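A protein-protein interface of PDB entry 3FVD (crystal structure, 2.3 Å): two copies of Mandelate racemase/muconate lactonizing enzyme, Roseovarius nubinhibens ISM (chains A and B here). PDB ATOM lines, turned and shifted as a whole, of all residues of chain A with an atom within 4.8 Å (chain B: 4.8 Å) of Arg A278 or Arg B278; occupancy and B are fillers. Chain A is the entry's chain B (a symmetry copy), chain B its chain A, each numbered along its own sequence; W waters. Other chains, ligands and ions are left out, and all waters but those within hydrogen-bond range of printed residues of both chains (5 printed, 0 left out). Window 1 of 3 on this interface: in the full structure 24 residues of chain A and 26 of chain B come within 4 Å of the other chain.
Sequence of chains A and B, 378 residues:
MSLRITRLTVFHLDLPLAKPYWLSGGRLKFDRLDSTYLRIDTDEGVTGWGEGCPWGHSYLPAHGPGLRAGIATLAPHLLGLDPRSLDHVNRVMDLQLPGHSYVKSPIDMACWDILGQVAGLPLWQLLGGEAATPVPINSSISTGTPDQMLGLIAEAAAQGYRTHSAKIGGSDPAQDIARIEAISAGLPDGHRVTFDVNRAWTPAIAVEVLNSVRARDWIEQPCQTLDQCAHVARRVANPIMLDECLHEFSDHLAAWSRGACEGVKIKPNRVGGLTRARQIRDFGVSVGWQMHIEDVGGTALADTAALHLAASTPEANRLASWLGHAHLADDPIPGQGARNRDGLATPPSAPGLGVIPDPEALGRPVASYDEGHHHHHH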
ATOM      1  N   ASP A  87       0.149  -0.017  25.305  1.00  0.00           N
ATOM      2  CA  ASP A  87       1.555  -0.335  25.295  1.00  0.00           C
ATOM      3  C   ASP A  87       2.233   0.638  26.207  1.00  0.00           C
ATOM      4  O   ASP A  87       3.031   0.236  27.038  1.00  0.00           O
ATOM      5  CB  ASP A  87       2.150  -0.247  23.896  1.00  0.00           C
ATOM      6  CG  ASP A  87       1.697  -1.377  23.001  1.00  0.00           C
ATOM      7  OD1 ASP A  87       1.437  -2.490  23.514  1.00  0.00           O
ATOM      8  OD2 ASP A  87       1.610  -1.181  21.757  1.00  0.00           O
ATOM      9  N   TRP A 112      -7.743  -2.433  29.205  1.00  0.00           N
ATOM     10  CA  TRP A 112      -8.324  -3.039  28.008  1.00  0.00           C
ATOM     11  C   TRP A 112      -9.854  -2.904  28.016  1.00  0.00           C
ATOM     12  O   TRP A 112     -10.460  -2.606  26.964  1.00  0.00           O
ATOM     13  CB  TRP A 112      -7.926  -4.508  27.875  1.00  0.00           C
ATOM     14  CG  TRP A 112      -6.706  -4.757  27.108  1.00  0.00           C
ATOM     15  CD1 TRP A 112      -5.445  -4.926  27.608  1.00  0.00           C
ATOM     16  CD2 TRP A 112      -6.601  -4.933  25.694  1.00  0.00           C
ATOM     17  NE1 TRP A 112      -4.557  -5.196  26.601  1.00  0.00           N
ATOM     18  CE2 TRP A 112      -5.230  -5.217  25.410  1.00  0.00           C
ATOM     19  CE3 TRP A 112      -7.525  -4.854  24.626  1.00  0.00           C
ATOM     20  CZ2 TRP A 112      -4.749  -5.432  24.115  1.00  0.00           C
ATOM     21  CZ3 TRP A 112      -7.060  -5.064  23.324  1.00  0.00           C
ATOM     22  CH2 TRP A 112      -5.659  -5.346  23.073  1.00  0.00           C
ATOM     23  N   LEU A 126     -11.105  -6.590  19.400  1.00  0.00           N
ATOM     24  CA  LEU A 126      -9.898  -5.787  19.449  1.00  0.00           C
ATOM     25  C   LEU A 126      -8.716  -6.711  19.379  1.00  0.00           C
ATOM     26  O   LEU A 126      -7.676  -6.327  18.875  1.00  0.00           O
ATOM     27  CB  LEU A 126      -9.825  -5.007  20.746  1.00  0.00           C
ATOM     28  CG  LEU A 126     -10.776  -3.819  20.759  1.00  0.00           C
ATOM     29  CD1 LEU A 126     -10.767  -3.207  22.121  1.00  0.00           C
ATOM     30  CD2 LEU A 126     -10.347  -2.782  19.702  1.00  0.00           C
ATOM     31  N   LEU A 127      -8.890  -7.933  19.872  1.00  0.00           N
ATOM     32  CA  LEU A 127      -7.868  -8.942  19.748  1.00  0.00           C
ATOM     33  C   LEU A 127      -7.880  -9.633  18.422  1.00  0.00           C
ATOM     34  O   LEU A 127      -7.192 -10.601  18.237  1.00  0.00           O
ATOM     35  CB  LEU A 127      -7.931  -9.965  20.884  1.00  0.00           C
ATOM     36  CG  LEU A 127      -7.632  -9.294  22.215  1.00  0.00           C
ATOM     37  CD1 LEU A 127      -8.102 -10.185  23.370  1.00  0.00           C
ATOM     38  CD2 LEU A 127      -6.140  -8.902  22.322  1.00  0.00           C
ATOM     39  N   LEU A 274      -3.073  -8.813  29.289  1.00  0.00           N
ATOM     40  CA  LEU A 274      -3.571  -9.127  27.989  1.00  0.00           C
ATOM     41  C   LEU A 274      -2.649  -8.621  26.908  1.00  0.00           C
ATOM     42  O   LEU A 274      -2.481  -9.244  25.885  1.00  0.00           O
ATOM     43  CB  LEU A 274      -4.937  -8.443  27.819  1.00  0.00           C
ATOM     44  CG  LEU A 274      -6.149  -9.324  27.695  1.00  0.00           C
ATOM     45  CD1 LEU A 274      -5.831 -10.763  28.140  1.00  0.00           C
ATOM     46  CD2 LEU A 274      -7.257  -8.671  28.497  1.00  0.00           C
ATOM     47  N   THR A 275      -2.034  -7.479  27.143  1.00  0.00           N
ATOM     48  CA  THR A 275      -1.143  -6.897  26.141  1.00  0.00           C
ATOM     49  C   THR A 275       0.033  -7.849  25.978  1.00  0.00           C
ATOM     50  O   THR A 275       0.385  -8.245  24.879  1.00  0.00           O
ATOM     51  CB  THR A 275      -0.667  -5.507  26.642  1.00  0.00           C
ATOM     52  OG1 THR A 275      -1.819  -4.628  26.787  1.00  0.00           O
ATOM     53  CG2 THR A 275       0.439  -4.914  25.719  1.00  0.00           C
ATOM     54  N   ARG A 276       0.629  -8.242  27.093  1.00  0.00           N
ATOM     55  CA  ARG A 276       1.731  -9.174  26.980  1.00  0.00           C
ATOM     56  C   ARG A 276       1.268 -10.574  26.498  1.00  0.00           C
ATOM     57  O   ARG A 276       1.997 -11.273  25.788  1.00  0.00           O
ATOM     58  CB  ARG A 276       2.455  -9.288  28.324  1.00  0.00           C
ATOM     59  CG  ARG A 276       3.168  -7.981  28.829  1.00  0.00           C
ATOM     60  CD  ARG A 276       4.607  -7.751  28.286  1.00  0.00           C
ATOM     61  NE  ARG A 276       5.147  -6.454  28.727  1.00  0.00           N
ATOM     62  CZ  ARG A 276       4.986  -5.283  28.057  1.00  0.00           C
ATOM     63  NH1 ARG A 276       5.492  -4.162  28.544  1.00  0.00           N
ATOM     64  NH2 ARG A 276       4.304  -5.216  26.901  1.00  0.00           N
ATOM     65  N   ALA A 277       0.065 -10.994  26.898  1.00  0.00           N
ATOM     66  CA  ALA A 277      -0.440 -12.333  26.513  1.00  0.00           C
ATOM     67  C   ALA A 277      -0.697 -12.349  25.040  1.00  0.00           C
ATOM     68  O   ALA A 277      -0.395 -13.295  24.351  1.00  0.00           O
ATOM     69  CB  ALA A 277      -1.707 -12.710  27.333  1.00  0.00           C
ATOM     70  N   ARG A 278      -1.104 -11.226  24.517  1.00  0.00           N
ATOM     71  CA  ARG A 278      -1.448 -11.193  23.129  1.00  0.00           C
ATOM     72  C   ARG A 278      -0.213 -11.310  22.254  1.00  0.00           C
ATOM     73  O   ARG A 278      -0.223 -11.954  21.217  1.00  0.00           O
ATOM     74  CB  ARG A 278      -2.206  -9.907  22.826  1.00  0.00           C
ATOM     75  CG  ARG A 278      -2.792  -9.946  21.439  1.00  0.00           C
ATOM     76  CD  ARG A 278      -1.960  -9.118  20.518  1.00  0.00           C
ATOM     77  NE  ARG A 278      -2.133  -7.716  20.808  1.00  0.00           N
ATOM     78  CZ  ARG A 278      -3.051  -6.920  20.236  1.00  0.00           C
ATOM     79  NH1 ARG A 278      -3.895  -7.418  19.303  1.00  0.00           N
ATOM     80  NH2 ARG A 278      -3.088  -5.606  20.570  1.00  0.00           N
ATOM     81  N   GLN A 279       0.852 -10.642  22.634  1.00  0.00           N
ATOM     82  CA  GLN A 279       2.092 -10.711  21.852  1.00  0.00           C
ATOM     83  C   GLN A 279       2.606 -12.157  21.795  1.00  0.00           C
ATOM     84  O   GLN A 279       3.107 -12.623  20.760  1.00  0.00           O
ATOM     85  CB  GLN A 279       3.167  -9.766  22.470  1.00  0.00           C
ATOM     86  CG  GLN A 279       4.622  -9.962  21.759  1.00  0.00           C
ATOM     87  CD  GLN A 279       5.871  -9.149  22.389  1.00  0.00           C
ATOM     88  OE1 GLN A 279       6.770  -8.792  21.635  1.00  0.00           O
ATOM     89  NE2 GLN A 279       5.923  -8.932  23.722  1.00  0.00           N
ATOM     90  N   ILE A 280       2.517 -12.858  22.909  1.00  0.00           N
ATOM     91  CA  ILE A 280       2.938 -14.280  22.982  1.00  0.00           C
ATOM     92  C   ILE A 280       2.020 -15.185  22.129  1.00  0.00           C
ATOM     93  O   ILE A 280       2.498 -16.110  21.427  1.00  0.00           O
ATOM     94  CB  ILE A 280       2.934 -14.747  24.475  1.00  0.00           C
ATOM     95  CG1 ILE A 280       4.041 -14.011  25.247  1.00  0.00           C
ATOM     96  CG2 ILE A 280       3.042 -16.277  24.597  1.00  0.00           C
ATOM     97  CD1 ILE A 280       3.731 -13.940  26.710  1.00  0.00           C
ATOM     98  N   ARG A 281       0.721 -14.876  22.160  1.00  0.00           N
ATOM     99  CA  ARG A 281      -0.260 -15.624  21.395  1.00  0.00           C
ATOM    100  C   ARG A 281       0.099 -15.545  19.951  1.00  0.00           C
ATOM    101  O   ARG A 281       0.169 -16.572  19.232  1.00  0.00           O
ATOM    102  CB  ARG A 281      -1.691 -15.028  21.604  1.00  0.00           C
ATOM    103  CG  ARG A 281      -2.835 -15.870  20.994  1.00  0.00           C
ATOM    104  CD  ARG A 281      -3.077 -15.513  19.524  1.00  0.00           C
ATOM    105  NE  ARG A 281      -3.418 -14.077  19.293  1.00  0.00           N
ATOM    106  CZ  ARG A 281      -4.639 -13.595  19.530  1.00  0.00           C
ATOM    107  NH1 ARG A 281      -5.582 -14.404  20.051  1.00  0.00           N
ATOM    108  NH2 ARG A 281      -4.933 -12.319  19.308  1.00  0.00           N
ATOM    109  N   ASP A 282       0.300 -14.308  19.503  1.00  0.00           N
ATOM    110  CA  ASP A 282       0.664 -14.094  18.112  1.00  0.00           C
ATOM    111  C   ASP A 282       1.967 -14.707  17.721  1.00  0.00           C
ATOM    112  O   ASP A 282       2.141 -15.115  16.596  1.00  0.00           O
ATOM    113  CB  ASP A 282       0.755 -12.584  17.837  1.00  0.00           C
ATOM    114  CG  ASP A 282      -0.620 -11.912  17.761  1.00  0.00           C
ATOM    115  OD1 ASP A 282      -1.725 -12.537  17.876  1.00  0.00           O
ATOM    116  OD2 ASP A 282      -0.575 -10.702  17.543  1.00  0.00           O
ATOM    117  N   LEU A 309      -9.138 -13.760  24.693  1.00  0.00           N
ATOM    118  CA  LEU A 309      -7.902 -13.977  23.942  1.00  0.00           C
ATOM    119  C   LEU A 309      -8.029 -15.335  23.337  1.00  0.00           C
ATOM    120  O   LEU A 309      -7.659 -15.555  22.214  1.00  0.00           O
ATOM    121  CB  LEU A 309      -6.615 -13.932  24.855  1.00  0.00           C
ATOM    122  CG  LEU A 309      -5.247 -13.955  24.126  1.00  0.00           C
ATOM    123  CD1 LEU A 309      -5.119 -12.829  23.113  1.00  0.00           C
ATOM    124  CD2 LEU A 309      -4.081 -13.887  25.104  1.00  0.00           C
ATOM    125  N   TRP B 112      -7.413  -0.678   8.991  1.00  0.00           N
ATOM    126  CA  TRP B 112      -6.962   0.046  10.178  1.00  0.00           C
ATOM    127  C   TRP B 112      -7.616   1.462  10.254  1.00  0.00           C
ATOM    128  O   TRP B 112      -8.010   1.950  11.336  1.00  0.00           O
ATOM    129  CB  TRP B 112      -5.446   0.159  10.161  1.00  0.00           C
ATOM    130  CG  TRP B 112      -4.728  -0.933  10.831  1.00  0.00           C
ATOM    131  CD1 TRP B 112      -4.170  -2.049  10.257  1.00  0.00           C
ATOM    132  CD2 TRP B 112      -4.407  -0.989  12.226  1.00  0.00           C
ATOM    133  NE1 TRP B 112      -3.562  -2.809  11.235  1.00  0.00           N
ATOM    134  CE2 TRP B 112      -3.706  -2.172  12.445  1.00  0.00           C
ATOM    135  CE3 TRP B 112      -4.699  -0.165  13.307  1.00  0.00           C
ATOM    136  CZ2 TRP B 112      -3.263  -2.541  13.700  1.00  0.00           C
ATOM    137  CZ3 TRP B 112      -4.295  -0.539  14.565  1.00  0.00           C
ATOM    138  CH2 TRP B 112      -3.554  -1.688  14.752  1.00  0.00           C
ATOM    139  N   LEU B 126      -4.073   3.555  18.833  1.00  0.00           N
ATOM    140  CA  LEU B 126      -4.371   2.111  18.676  1.00  0.00           C
ATOM    141  C   LEU B 126      -3.068   1.239  18.604  1.00  0.00           C
ATOM    142  O   LEU B 126      -3.065   0.071  18.986  1.00  0.00           O
ATOM    143  CB  LEU B 126      -5.145   1.877  17.386  1.00  0.00           C
ATOM    144  CG  LEU B 126      -6.611   2.325  17.471  1.00  0.00           C
ATOM    145  CD1 LEU B 126      -7.265   2.220  16.120  1.00  0.00           C
ATOM    146  CD2 LEU B 126      -7.349   1.466  18.453  1.00  0.00           C
ATOM    147  N   LEU B 127      -1.992   1.807  18.073  1.00  0.00           N
ATOM    148  CA  LEU B 127      -0.704   1.132  18.027  1.00  0.00           C
ATOM    149  C   LEU B 127       0.045   1.363  19.328  1.00  0.00           C
ATOM    150  O   LEU B 127       1.209   1.047  19.445  1.00  0.00           O
ATOM    151  CB  LEU B 127       0.108   1.596  16.808  1.00  0.00           C
ATOM    152  CG  LEU B 127      -0.562   1.162  15.476  1.00  0.00           C
ATOM    153  CD1 LEU B 127      -0.165   2.030  14.304  1.00  0.00           C
ATOM    154  CD2 LEU B 127      -0.132  -0.220  15.207  1.00  0.00           C
ATOM    155  N   LEU B 274       0.045  -2.820   8.183  1.00  0.00           N
ATOM    156  CA  LEU B 274       0.242  -2.360   9.541  1.00  0.00           C
ATOM    157  C   LEU B 274       0.148  -3.471  10.555  1.00  0.00           C
ATOM    158  O   LEU B 274       0.868  -3.414  11.545  1.00  0.00           O
ATOM    159  CB  LEU B 274      -0.734  -1.244   9.926  1.00  0.00           C
ATOM    160  CG  LEU B 274      -0.457   0.094   9.288  1.00  0.00           C
ATOM    161  CD1 LEU B 274      -1.486   1.022   9.874  1.00  0.00           C
ATOM    162  CD2 LEU B 274       0.979   0.547   9.669  1.00  0.00           C
ATOM    163  N   THR B 275      -0.706  -4.487  10.311  1.00  0.00           N
ATOM    164  CA  THR B 275      -0.876  -5.521  11.342  1.00  0.00           C
ATOM    165  C   THR B 275       0.399  -6.364  11.434  1.00  0.00           C
ATOM    166  O   THR B 275       0.895  -6.627  12.484  1.00  0.00           O
ATOM    167  CB  THR B 275      -2.080  -6.445  11.050  1.00  0.00           C
ATOM    168  OG1 THR B 275      -3.268  -5.635  11.007  1.00  0.00           O
ATOM    169  CG2 THR B 275      -2.205  -7.555  12.113  1.00  0.00           C
ATOM    170  N   ARG B 276       0.936  -6.756  10.302  1.00  0.00           N
ATOM    171  CA  ARG B 276       2.182  -7.474  10.290  1.00  0.00           C
ATOM    172  C   ARG B 276       3.289  -6.592  10.791  1.00  0.00           C
ATOM    173  O   ARG B 276       4.172  -7.074  11.473  1.00  0.00           O
ATOM    174  CB  ARG B 276       2.466  -7.924   8.863  1.00  0.00           C
ATOM    175  CG  ARG B 276       1.431  -8.926   8.395  1.00  0.00           C
ATOM    176  CD  ARG B 276       1.622 -10.267   9.107  1.00  0.00           C
ATOM    177  NE  ARG B 276       0.691 -11.229   8.553  1.00  0.00           N
ATOM    178  CZ  ARG B 276      -0.410 -11.643   9.168  1.00  0.00           C
ATOM    179  NH1 ARG B 276      -1.203 -12.509   8.541  1.00  0.00           N
ATOM    180  NH2 ARG B 276      -0.706 -11.200  10.406  1.00  0.00           N
ATOM    181  N   ALA B 277       3.270  -5.295  10.450  1.00  0.00           N
ATOM    182  CA  ALA B 277       4.432  -4.394  10.829  1.00  0.00           C
ATOM    183  C   ALA B 277       4.477  -4.218  12.325  1.00  0.00           C
ATOM    184  O   ALA B 277       5.546  -4.208  12.986  1.00  0.00           O
ATOM    185  CB  ALA B 277       4.334  -2.981  10.037  1.00  0.00           C
ATOM    186  N   ARG B 278       3.306  -4.210  12.926  1.00  0.00           N
ATOM    187  CA  ARG B 278       3.230  -3.965  14.357  1.00  0.00           C
ATOM    188  C   ARG B 278       3.766  -5.145  15.150  1.00  0.00           C
ATOM    189  O   ARG B 278       4.416  -4.990  16.193  1.00  0.00           O
ATOM    190  CB  ARG B 278       1.794  -3.653  14.741  1.00  0.00           C
ATOM    191  CG  ARG B 278       1.717  -3.224  16.143  1.00  0.00           C
ATOM    192  CD  ARG B 278       1.181  -4.335  16.999  1.00  0.00           C
ATOM    193  NE  ARG B 278      -0.261  -4.528  16.843  1.00  0.00           N
ATOM    194  CZ  ARG B 278      -1.174  -3.903  17.590  1.00  0.00           C
ATOM    195  NH1 ARG B 278      -2.454  -4.190  17.379  1.00  0.00           N
ATOM    196  NH2 ARG B 278      -0.823  -3.007  18.548  1.00  0.00           N
ATOM    197  N   GLN B 279       3.470  -6.344  14.660  1.00  0.00           N
ATOM    198  CA  GLN B 279       3.976  -7.558  15.283  1.00  0.00           C
ATOM    199  C   GLN B 279       5.509  -7.513  15.199  1.00  0.00           C
ATOM    200  O   GLN B 279       6.182  -7.814  16.178  1.00  0.00           O
ATOM    201  CB  GLN B 279       3.378  -8.849  14.616  1.00  0.00           C
ATOM    202  CG  GLN B 279       3.958 -10.135  15.272  1.00  0.00           C
ATOM    203  CD  GLN B 279       3.642 -11.529  14.573  1.00  0.00           C
ATOM    204  OE1 GLN B 279       3.707 -12.563  15.262  1.00  0.00           O
ATOM    205  NE2 GLN B 279       3.383 -11.552  13.248  1.00  0.00           N
ATOM    206  N   ILE B 280       6.063  -7.129  14.037  1.00  0.00           N
ATOM    207  CA  ILE B 280       7.529  -7.007  13.913  1.00  0.00           C
ATOM    208  C   ILE B 280       8.107  -5.946  14.840  1.00  0.00           C
ATOM    209  O   ILE B 280       9.087  -6.185  15.546  1.00  0.00           O
ATOM    210  CB  ILE B 280       7.964  -6.726  12.452  1.00  0.00           C
ATOM    211  CG1 ILE B 280       7.567  -7.961  11.605  1.00  0.00           C
ATOM    212  CG2 ILE B 280       9.496  -6.498  12.422  1.00  0.00           C
ATOM    213  CD1 ILE B 280       7.379  -7.685  10.106  1.00  0.00           C
ATOM    214  N   ARG B 281       7.461  -4.774  14.860  1.00  0.00           N
ATOM    215  CA  ARG B 281       7.885  -3.692  15.732  1.00  0.00           C
ATOM    216  C   ARG B 281       7.928  -4.149  17.209  1.00  0.00           C
ATOM    217  O   ARG B 281       8.952  -3.933  17.904  1.00  0.00           O
ATOM    218  CB  ARG B 281       6.981  -2.432  15.494  1.00  0.00           C
ATOM    219  CG  ARG B 281       7.348  -1.171  16.323  1.00  0.00           C
ATOM    220  CD  ARG B 281       7.009  -1.286  17.770  1.00  0.00           C
ATOM    221  NE  ARG B 281       5.588  -1.389  18.091  1.00  0.00           N
ATOM    222  CZ  ARG B 281       4.718  -0.381  18.032  1.00  0.00           C
ATOM    223  NH1 ARG B 281       5.087   0.803  17.567  1.00  0.00           N
ATOM    224  NH2 ARG B 281       3.450  -0.559  18.372  1.00  0.00           N
ATOM    225  N   ASP B 282       6.868  -4.825  17.682  1.00  0.00           N
ATOM    226  CA  ASP B 282       6.873  -5.274  19.072  1.00  0.00           C
ATOM    227  C   ASP B 282       8.012  -6.283  19.314  1.00  0.00           C
ATOM    228  O   ASP B 282       8.600  -6.335  20.390  1.00  0.00           O
ATOM    229  CB  ASP B 282       5.506  -5.880  19.492  1.00  0.00           C
ATOM    230  CG  ASP B 282       4.363  -4.824  19.586  1.00  0.00           C
ATOM    231  OD1 ASP B 282       4.558  -3.586  19.400  1.00  0.00           O
ATOM    232  OD2 ASP B 282       3.219  -5.211  19.843  1.00  0.00           O
ATOM    233  N   LEU B 309       2.970   4.273  13.122  1.00  0.00           N
ATOM    234  CA  LEU B 309       3.637   3.155  13.781  1.00  0.00           C
ATOM    235  C   LEU B 309       4.971   3.640  14.293  1.00  0.00           C
ATOM    236  O   LEU B 309       5.349   3.296  15.432  1.00  0.00           O
ATOM    237  CB  LEU B 309       3.813   1.961  12.814  1.00  0.00           C
ATOM    238  CG  LEU B 309       4.497   0.723  13.438  1.00  0.00           C
ATOM    239  CD1 LEU B 309       3.660   0.087  14.544  1.00  0.00           C
ATOM    240  CD2 LEU B 309       4.801  -0.301  12.352  1.00  0.00           C
HETATM  241  O   HOH W   1       1.845  -2.468  19.523  1.00  0.00           O
HETATM  242  O   HOH W   2       7.294  -5.553  22.669  1.00  0.00           O
HETATM  243  O   HOH W   3       3.782   1.408  21.358  1.00  0.00           O
HETATM  244  O   HOH W   4       5.923  -9.532  18.657  1.00  0.00           O
HETATM  245  O   HOH W   5       4.307 -11.640  18.312  1.00  0.00           O
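OE1 of Gln A279 sits close to O of Asp B282, at 3.3 Å.
The side-chain carboxylate (OD2) of Asp A87 lies close to the backbone carbonyl oxygen (O) of Leu B127, at 3.2 Å.
NH2 of Arg B281 lies within salt-bridge range of OD2 of Asp A87, 3.9 Å away.
OE1 of Gln B279 sits close to O of Asp A282 (3.3 Å).
NE of Arg A281 lies within salt-bridge range of OD1 of Asp A282 (2.7 Å).
NH2 of Arg B281 sits at hydrogen-bond distance from O of Leu B127 (3.0 Å).
OD1 of Asp B282 is in salt-bridge range of NE of Arg B281.
O of Leu B309 is in hydrogen-bond range of NH1 of Arg B281 (3.3 Å).
Among the printed residues, merely in contact across the chains: Arg A278 with Arg B278.
Printed residues of chain B within 4 Å of Asp A87: Leu B127 (3.2 Å) and Arg B281 (3.9 Å).
Of chain B, only Arg B278 comes within 4 Å of Arg A278.
Printed residues of chain B within 4 Å of Asp A282: Gln B279 (3.3 Å).
Of chain A, only Arg A278 comes within 4 Å of Arg B278.
Ile B280 touches none of the printed residues of chain A.
The nearest printed residue of chain B that does not touch Arg A278 is Leu B126 (5.9 Å).
The nearest residue of chain A that does not touch Arg B278 is Asp A87 (4.4 Å).
The nearest printed residue of chain B that does not touch Asp A282 is Arg B278 (6.2 Å).
Arg B278 touches its own counterpart, Arg A278.
Gln A279 touches Asp B282, and with the chains exchanged Asp A282 touches Gln B279.
Positions printed for both chains: 112, 126, 127, 274, 275, 276, 277, 278, 279, 280, 281, 282 and 309.
Water W1 lies within hydrogen-bond range of OD2 of Asp A87, NH2 of Arg B281, NH2 of Arg B278 and OD1 of Asp B282.
Water W2 bridges O of Asp B282 (2.7 Å) and OE1 of Gln A279 (3.4 Å).
Water W5 lies within hydrogen-bond range of the backbone carbonyl oxygen (O) of Gln A279 (2.9 Å) and the side-chain amide oxygen (OE1) of Gln B279 (3.2 Å).
Water W4 bridges the backbone carbonyl oxygen (O) of Gln B279 (3.0 Å) and the side-chain amide oxygen (OE1) of Gln A279 (3.2 Å).
Water W3 lies within hydrogen-bond range of the backbone carbonyl oxygen of Leu B127 (3.2 Å) and the side-chain carboxylate of Asp A87 (3.4 Å).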
